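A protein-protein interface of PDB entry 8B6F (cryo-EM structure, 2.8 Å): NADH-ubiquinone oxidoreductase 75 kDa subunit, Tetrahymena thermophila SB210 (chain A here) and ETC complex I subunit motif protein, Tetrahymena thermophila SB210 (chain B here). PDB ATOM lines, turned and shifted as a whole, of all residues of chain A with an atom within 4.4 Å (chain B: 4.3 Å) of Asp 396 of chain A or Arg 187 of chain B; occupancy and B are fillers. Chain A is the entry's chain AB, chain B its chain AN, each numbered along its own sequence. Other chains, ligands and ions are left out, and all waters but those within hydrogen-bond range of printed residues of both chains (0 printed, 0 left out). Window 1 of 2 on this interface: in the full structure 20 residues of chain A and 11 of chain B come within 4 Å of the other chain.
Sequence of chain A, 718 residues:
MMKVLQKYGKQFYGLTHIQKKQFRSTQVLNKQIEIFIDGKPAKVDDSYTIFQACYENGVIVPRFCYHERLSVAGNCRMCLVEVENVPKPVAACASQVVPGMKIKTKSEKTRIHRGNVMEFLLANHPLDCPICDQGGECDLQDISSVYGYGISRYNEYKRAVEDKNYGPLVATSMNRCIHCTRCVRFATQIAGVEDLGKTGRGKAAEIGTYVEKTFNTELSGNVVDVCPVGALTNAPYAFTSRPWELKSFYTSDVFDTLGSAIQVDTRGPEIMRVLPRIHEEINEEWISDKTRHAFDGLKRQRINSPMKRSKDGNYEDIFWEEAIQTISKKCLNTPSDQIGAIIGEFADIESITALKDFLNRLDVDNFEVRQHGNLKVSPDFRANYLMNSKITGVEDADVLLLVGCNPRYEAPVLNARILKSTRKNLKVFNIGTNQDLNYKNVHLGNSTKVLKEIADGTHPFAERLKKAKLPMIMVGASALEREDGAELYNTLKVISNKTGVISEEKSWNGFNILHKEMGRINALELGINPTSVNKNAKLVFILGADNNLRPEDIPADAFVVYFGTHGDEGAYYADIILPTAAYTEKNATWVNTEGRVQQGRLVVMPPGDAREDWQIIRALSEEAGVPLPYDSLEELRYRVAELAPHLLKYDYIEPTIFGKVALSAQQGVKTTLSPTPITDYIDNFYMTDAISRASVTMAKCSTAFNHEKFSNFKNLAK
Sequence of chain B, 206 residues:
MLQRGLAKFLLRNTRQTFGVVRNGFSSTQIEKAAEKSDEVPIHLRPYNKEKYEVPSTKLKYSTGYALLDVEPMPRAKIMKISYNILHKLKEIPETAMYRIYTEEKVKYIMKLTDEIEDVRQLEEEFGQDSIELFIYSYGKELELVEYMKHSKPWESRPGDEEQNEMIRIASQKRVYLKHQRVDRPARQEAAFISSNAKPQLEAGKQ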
ATOM      1  N   THR A 392     -20.792 -19.443 -17.391  1.00  0.00           N
ATOM      2  CA  THR A 392     -19.822 -18.369 -17.233  1.00  0.00           C
ATOM      3  C   THR A 392     -20.206 -17.108 -17.992  1.00  0.00           C
ATOM      4  O   THR A 392     -19.455 -16.128 -17.952  1.00  0.00           O
ATOM      5  CB  THR A 392     -18.442 -18.838 -17.696  1.00  0.00           C
ATOM      6  OG1 THR A 392     -18.509 -19.248 -19.068  1.00  0.00           O
ATOM      7  CG2 THR A 392     -17.958 -19.999 -16.843  1.00  0.00           C
ATOM      8  N   GLY A 393     -21.345 -17.109 -18.685  1.00  0.00           N
ATOM      9  CA  GLY A 393     -21.766 -15.937 -19.427  1.00  0.00           C
ATOM     10  C   GLY A 393     -22.201 -14.782 -18.554  1.00  0.00           C
ATOM     11  O   GLY A 393     -22.199 -13.636 -19.014  1.00  0.00           O
ATOM     12  N   VAL A 394     -22.578 -15.054 -17.304  1.00  0.00           N
ATOM     13  CA  VAL A 394     -22.910 -13.975 -16.381  1.00  0.00           C
ATOM     14  C   VAL A 394     -21.670 -13.151 -16.069  1.00  0.00           C
ATOM     15  O   VAL A 394     -21.746 -11.930 -15.890  1.00  0.00           O
ATOM     16  CB  VAL A 394     -23.559 -14.546 -15.106  1.00  0.00           C
ATOM     17  CG1 VAL A 394     -22.588 -15.448 -14.355  1.00  0.00           C
ATOM     18  CG2 VAL A 394     -24.053 -13.419 -14.216  1.00  0.00           C
ATOM     19  N   GLU A 395     -20.512 -13.804 -15.996  1.00  0.00           N
ATOM     20  CA  GLU A 395     -19.259 -13.099 -15.772  1.00  0.00           C
ATOM     21  C   GLU A 395     -18.875 -12.210 -16.947  1.00  0.00           C
ATOM     22  O   GLU A 395     -17.968 -11.384 -16.804  1.00  0.00           O
ATOM     23  CB  GLU A 395     -18.143 -14.109 -15.502  1.00  0.00           C
ATOM     24  CG  GLU A 395     -18.418 -15.018 -14.316  1.00  0.00           C
ATOM     25  CD  GLU A 395     -17.418 -16.149 -14.210  1.00  0.00           C
ATOM     26  OE1 GLU A 395     -16.552 -16.261 -15.101  1.00  0.00           O
ATOM     27  OE2 GLU A 395     -17.498 -16.928 -13.238  1.00  0.00           O
ATOM     28  N   ASP A 396     -19.532 -12.364 -18.097  1.00  0.00           N
ATOM     29  CA  ASP A 396     -19.248 -11.562 -19.281  1.00  0.00           C
ATOM     30  C   ASP A 396     -20.330 -10.544 -19.601  1.00  0.00           C
ATOM     31  O   ASP A 396     -20.021  -9.499 -20.176  1.00  0.00           O
ATOM     32  CB  ASP A 396     -19.060 -12.471 -20.501  1.00  0.00           C
ATOM     33  CG  ASP A 396     -17.973 -13.506 -20.293  1.00  0.00           C
ATOM     34  OD1 ASP A 396     -16.933 -13.164 -19.691  1.00  0.00           O
ATOM     35  OD2 ASP A 396     -18.161 -14.664 -20.722  1.00  0.00           O
ATOM     36  N   ALA A 397     -21.580 -10.820 -19.249  1.00  0.00           N
ATOM     37  CA  ALA A 397     -22.665  -9.894 -19.540  1.00  0.00           C
ATOM     38  C   ALA A 397     -22.598  -8.672 -18.631  1.00  0.00           C
ATOM     39  O   ALA A 397     -22.160  -8.746 -17.480  1.00  0.00           O
ATOM     40  CB  ALA A 397     -24.015 -10.588 -19.376  1.00  0.00           C
ATOM     41  N   ASP A 398     -23.041  -7.532 -19.165  1.00  0.00           N
ATOM     42  CA  ASP A 398     -23.113  -6.298 -18.392  1.00  0.00           C
ATOM     43  C   ASP A 398     -24.487  -6.069 -17.785  1.00  0.00           C
ATOM     44  O   ASP A 398     -24.589  -5.472 -16.707  1.00  0.00           O
ATOM     45  CB  ASP A 398     -22.741  -5.097 -19.265  1.00  0.00           C
ATOM     46  CG  ASP A 398     -21.305  -5.149 -19.750  1.00  0.00           C
ATOM     47  OD1 ASP A 398     -20.629  -6.168 -19.496  1.00  0.00           O
ATOM     48  OD2 ASP A 398     -20.851  -4.169 -20.378  1.00  0.00           O
ATOM     49  N   LEU A 470     -23.392  -6.865 -24.639  1.00  0.00           N
ATOM     50  CA  LEU A 470     -23.514  -8.238 -24.166  1.00  0.00           C
ATOM     51  C   LEU A 470     -24.602  -8.370 -23.096  1.00  0.00           C
ATOM     52  O   LEU A 470     -24.329  -8.817 -21.979  1.00  0.00           O
ATOM     53  CB  LEU A 470     -22.179  -8.750 -23.643  1.00  0.00           C
ATOM     54  CG  LEU A 470     -21.108  -9.074 -24.691  1.00  0.00           C
ATOM     55  CD1 LEU A 470     -20.616  -7.826 -25.410  1.00  0.00           C
ATOM     56  CD2 LEU A 470     -19.943  -9.813 -24.050  1.00  0.00           C
ATOM     57  N   LYS A 506     -21.230  -8.618 -32.233  1.00  0.00           N
ATOM     58  CA  LYS A 506     -20.678  -8.993 -30.939  1.00  0.00           C
ATOM     59  C   LYS A 506     -20.403 -10.485 -30.830  1.00  0.00           C
ATOM     60  O   LYS A 506     -19.728 -10.905 -29.884  1.00  0.00           O
ATOM     61  CB  LYS A 506     -21.634  -8.583 -29.818  1.00  0.00           C
ATOM     62  CG  LYS A 506     -21.977  -7.104 -29.789  1.00  0.00           C
ATOM     63  CD  LYS A 506     -23.078  -6.833 -28.775  1.00  0.00           C
ATOM     64  CE  LYS A 506     -23.477  -5.370 -28.760  1.00  0.00           C
ATOM     65  NZ  LYS A 506     -24.631  -5.130 -27.852  1.00  0.00           N
ATOM     66  N   SER A 507     -20.905 -11.289 -31.765  1.00  0.00           N
ATOM     67  CA  SER A 507     -20.790 -12.740 -31.678  1.00  0.00           C
ATOM     68  C   SER A 507     -21.307 -13.238 -30.333  1.00  0.00           C
ATOM     69  O   SER A 507     -20.707 -14.100 -29.689  1.00  0.00           O
ATOM     70  CB  SER A 507     -19.349 -13.190 -31.912  1.00  0.00           C
ATOM     71  OG  SER A 507     -19.250 -14.601 -31.863  1.00  0.00           O
ATOM     72  N   TRP A 508     -22.433 -12.678 -29.905  1.00  0.00           N
ATOM     73  CA  TRP A 508     -23.005 -12.937 -28.594  1.00  0.00           C
ATOM     74  C   TRP A 508     -24.439 -13.421 -28.746  1.00  0.00           C
ATOM     75  O   TRP A 508     -25.183 -12.931 -29.600  1.00  0.00           O
ATOM     76  CB  TRP A 508     -22.964 -11.677 -27.724  1.00  0.00           C
ATOM     77  CG  TRP A 508     -23.758 -11.785 -26.463  1.00  0.00           C
ATOM     78  CD1 TRP A 508     -24.979 -11.231 -26.217  1.00  0.00           C
ATOM     79  CD2 TRP A 508     -23.389 -12.493 -25.272  1.00  0.00           C
ATOM     80  NE1 TRP A 508     -25.394 -11.549 -24.947  1.00  0.00           N
ATOM     81  CE2 TRP A 508     -24.436 -12.321 -24.346  1.00  0.00           C
ATOM     82  CE3 TRP A 508     -22.276 -13.252 -24.902  1.00  0.00           C
ATOM     83  CZ2 TRP A 508     -24.402 -12.882 -23.072  1.00  0.00           C
ATOM     84  CZ3 TRP A 508     -22.244 -13.808 -23.635  1.00  0.00           C
ATOM     85  CH2 TRP A 508     -23.301 -13.621 -22.736  1.00  0.00           C
ATOM     86  N   ARG B 184      -8.182 -18.676 -16.788  1.00  0.00           N
ATOM     87  CA  ARG B 184      -9.582 -18.704 -17.185  1.00  0.00           C
ATOM     88  C   ARG B 184      -9.685 -18.426 -18.678  1.00  0.00           C
ATOM     89  O   ARG B 184      -9.212 -17.377 -19.135  1.00  0.00           O
ATOM     90  CB  ARG B 184     -10.377 -17.670 -16.396  1.00  0.00           C
ATOM     91  CG  ARG B 184     -11.864 -17.666 -16.712  1.00  0.00           C
ATOM     92  CD  ARG B 184     -12.589 -16.572 -15.950  1.00  0.00           C
ATOM     93  NE  ARG B 184     -14.016 -16.569 -16.246  1.00  0.00           N
ATOM     94  CZ  ARG B 184     -14.563 -15.991 -17.307  1.00  0.00           C
ATOM     95  NH1 ARG B 184     -13.828 -15.356 -18.206  1.00  0.00           N
ATOM     96  NH2 ARG B 184     -15.881 -16.053 -17.472  1.00  0.00           N
ATOM     97  N   PRO B 185     -10.281 -19.312 -19.474  1.00  0.00           N
ATOM     98  CA  PRO B 185     -10.378 -19.048 -20.912  1.00  0.00           C
ATOM     99  C   PRO B 185     -11.295 -17.873 -21.205  1.00  0.00           C
ATOM    100  O   PRO B 185     -12.236 -17.584 -20.462  1.00  0.00           O
ATOM    101  CB  PRO B 185     -10.945 -20.355 -21.479  1.00  0.00           C
ATOM    102  CG  PRO B 185     -11.677 -20.967 -20.345  1.00  0.00           C
ATOM    103  CD  PRO B 185     -10.915 -20.591 -19.108  1.00  0.00           C
ATOM    104  N   ALA B 186     -11.003 -17.189 -22.307  1.00  0.00           N
ATOM    105  CA  ALA B 186     -11.837 -16.082 -22.744  1.00  0.00           C
ATOM    106  C   ALA B 186     -13.177 -16.598 -23.262  1.00  0.00           C
ATOM    107  O   ALA B 186     -13.337 -17.778 -23.586  1.00  0.00           O
ATOM    108  CB  ALA B 186     -11.130 -15.277 -23.833  1.00  0.00           C
ATOM    109  N   ARG B 187     -14.149 -15.692 -23.332  1.00  0.00           N
ATOM    110  CA  ARG B 187     -15.472 -16.067 -23.809  1.00  0.00           C
ATOM    111  C   ARG B 187     -15.381 -16.661 -25.207  1.00  0.00           C
ATOM    112  O   ARG B 187     -14.673 -16.145 -26.076  1.00  0.00           O
ATOM    113  CB  ARG B 187     -16.400 -14.852 -23.813  1.00  0.00           C
ATOM    114  CG  ARG B 187     -17.809 -15.165 -24.291  1.00  0.00           C
ATOM    115  CD  ARG B 187     -18.707 -13.942 -24.236  1.00  0.00           C
ATOM    116  NE  ARG B 187     -18.266 -12.888 -25.144  1.00  0.00           N
ATOM    117  CZ  ARG B 187     -18.561 -12.837 -26.436  1.00  0.00           C
ATOM    118  NH1 ARG B 187     -19.278 -13.782 -27.020  1.00  0.00           N
ATOM    119  NH2 ARG B 187     -18.126 -11.810 -27.160  1.00  0.00           N
ATOM    120  N   GLN B 188     -16.099 -17.760 -25.420  1.00  0.00           N
ATOM    121  CA  GLN B 188     -16.131 -18.395 -26.732  1.00  0.00           C
ATOM    122  C   GLN B 188     -16.993 -17.569 -27.675  1.00  0.00           C
ATOM    123  O   GLN B 188     -18.169 -17.315 -27.394  1.00  0.00           O
ATOM    124  CB  GLN B 188     -16.666 -19.821 -26.621  1.00  0.00           C
ATOM    125  CG  GLN B 188     -15.778 -20.750 -25.814  1.00  0.00           C
ATOM    126  CD  GLN B 188     -16.261 -22.184 -25.845  1.00  0.00           C
ATOM    127  OE1 GLN B 188     -17.176 -22.527 -26.592  1.00  0.00           O
ATOM    128  NE2 GLN B 188     -15.647 -23.032 -25.028  1.00  0.00           N
ATOM    129  N   GLU B 189     -16.412 -17.156 -28.796  1.00  0.00           N
ATOM    130  CA  GLU B 189     -17.126 -16.322 -29.753  1.00  0.00           C
ATOM    131  C   GLU B 189     -18.198 -17.146 -30.455  1.00  0.00           C
ATOM    132  O   GLU B 189     -17.884 -18.100 -31.174  1.00  0.00           O
ATOM    133  CB  GLU B 189     -16.147 -15.738 -30.768  1.00  0.00           C
ATOM    134  CG  GLU B 189     -14.955 -15.028 -30.148  1.00  0.00           C
ATOM    135  CD  GLU B 189     -15.360 -13.863 -29.271  1.00  0.00           C
ATOM    136  OE1 GLU B 189     -16.525 -13.425 -29.363  1.00  0.00           O
ATOM    137  OE2 GLU B 189     -14.514 -13.386 -28.486  1.00  0.00           O
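NH2 of Arg 184 of chain B is in salt-bridge range of OE1 of Glu 395 of chain A (2.5 Å). The side-chain carboxylate of Asp 396 of chain A is in salt-bridge range of the guanidinium group of Arg 184 of chain B (3.8 Å). The backbone carbonyl oxygen (O) of Lys 506 of chain A sits at hydrogen-bond distance from the guanidinium group (NH2) of Arg 187 of chain B (3.3 Å). NH1 of Arg 187 of chain B sits at hydrogen-bond distance from O of Ser 507 of chain A (3.0 Å).
The backbone carbonyl oxygen (O) of Leu 470 of chain A lies within hydrogen-bond range of the backbone NH (N) of Asp 398 of chain A (3.4 Å). The side-chain carboxylate (OE1) of Glu 189 of chain B lies within salt-bridge range of the guanidinium group (NH2) of Arg 187 of chain B, at 3.2 Å.
Among the printed residues, pairs that only touch across the chains: Thr 392 of chain A with Arg 184 of chain B, Asp 396 of chain A with Arg 187 of chain B, Leu 470 of chain A with Arg 187 of chain B, Ser 507 of chain A with Glu 189 of chain B and Trp 508 of chain A with Arg 187 of chain B.
Of chain B, only Arg 184 and Arg 187 come within 4 Å of Asp 396 of chain A. Arg 187 of chain B touches five residues of chain A. Of the printed residues of chain B, Leu 470 of chain A touches Arg 187 (3.7 Å). Of the printed residues of chain B, Thr 392 of chain A touches Arg 184 (3.6 Å). Of the printed residues of chain B, Glu 395 of chain A touches Arg 184. Of the printed residues of chain A, Arg 184 of chain B touches Thr 392, Glu 395 and Asp 396. Printed residues of chain A within 4 Å of Glu 189 of chain B: Ser 507 (3.1 Å). Ala 397 of chain A touches none of the printed residues of chain B. The nearest printed residue of chain B that does not touch Asp 396 of chain A is Ala 186 of chain B (5.9 Å). The nearest printed residue of chain A that does not touch Arg 187 of chain B is Gly 393 of chain A (6.0 Å).
Of the 11 printed residues of chain A, 7 touch a printed residue of chain B. Hydrophobic or aromatic side chains of chain A within 4 Å of the printed part of chain B: Leu 470 and Trp 508. Among the printed residues, Asp or Glu carboxylates within 4 Å of a Lys or Arg side-chain nitrogen of the other chain: Glu 395 of chain A with Arg 184 of chain B and Asp 396 of chain A with Arg 184 of chain B.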
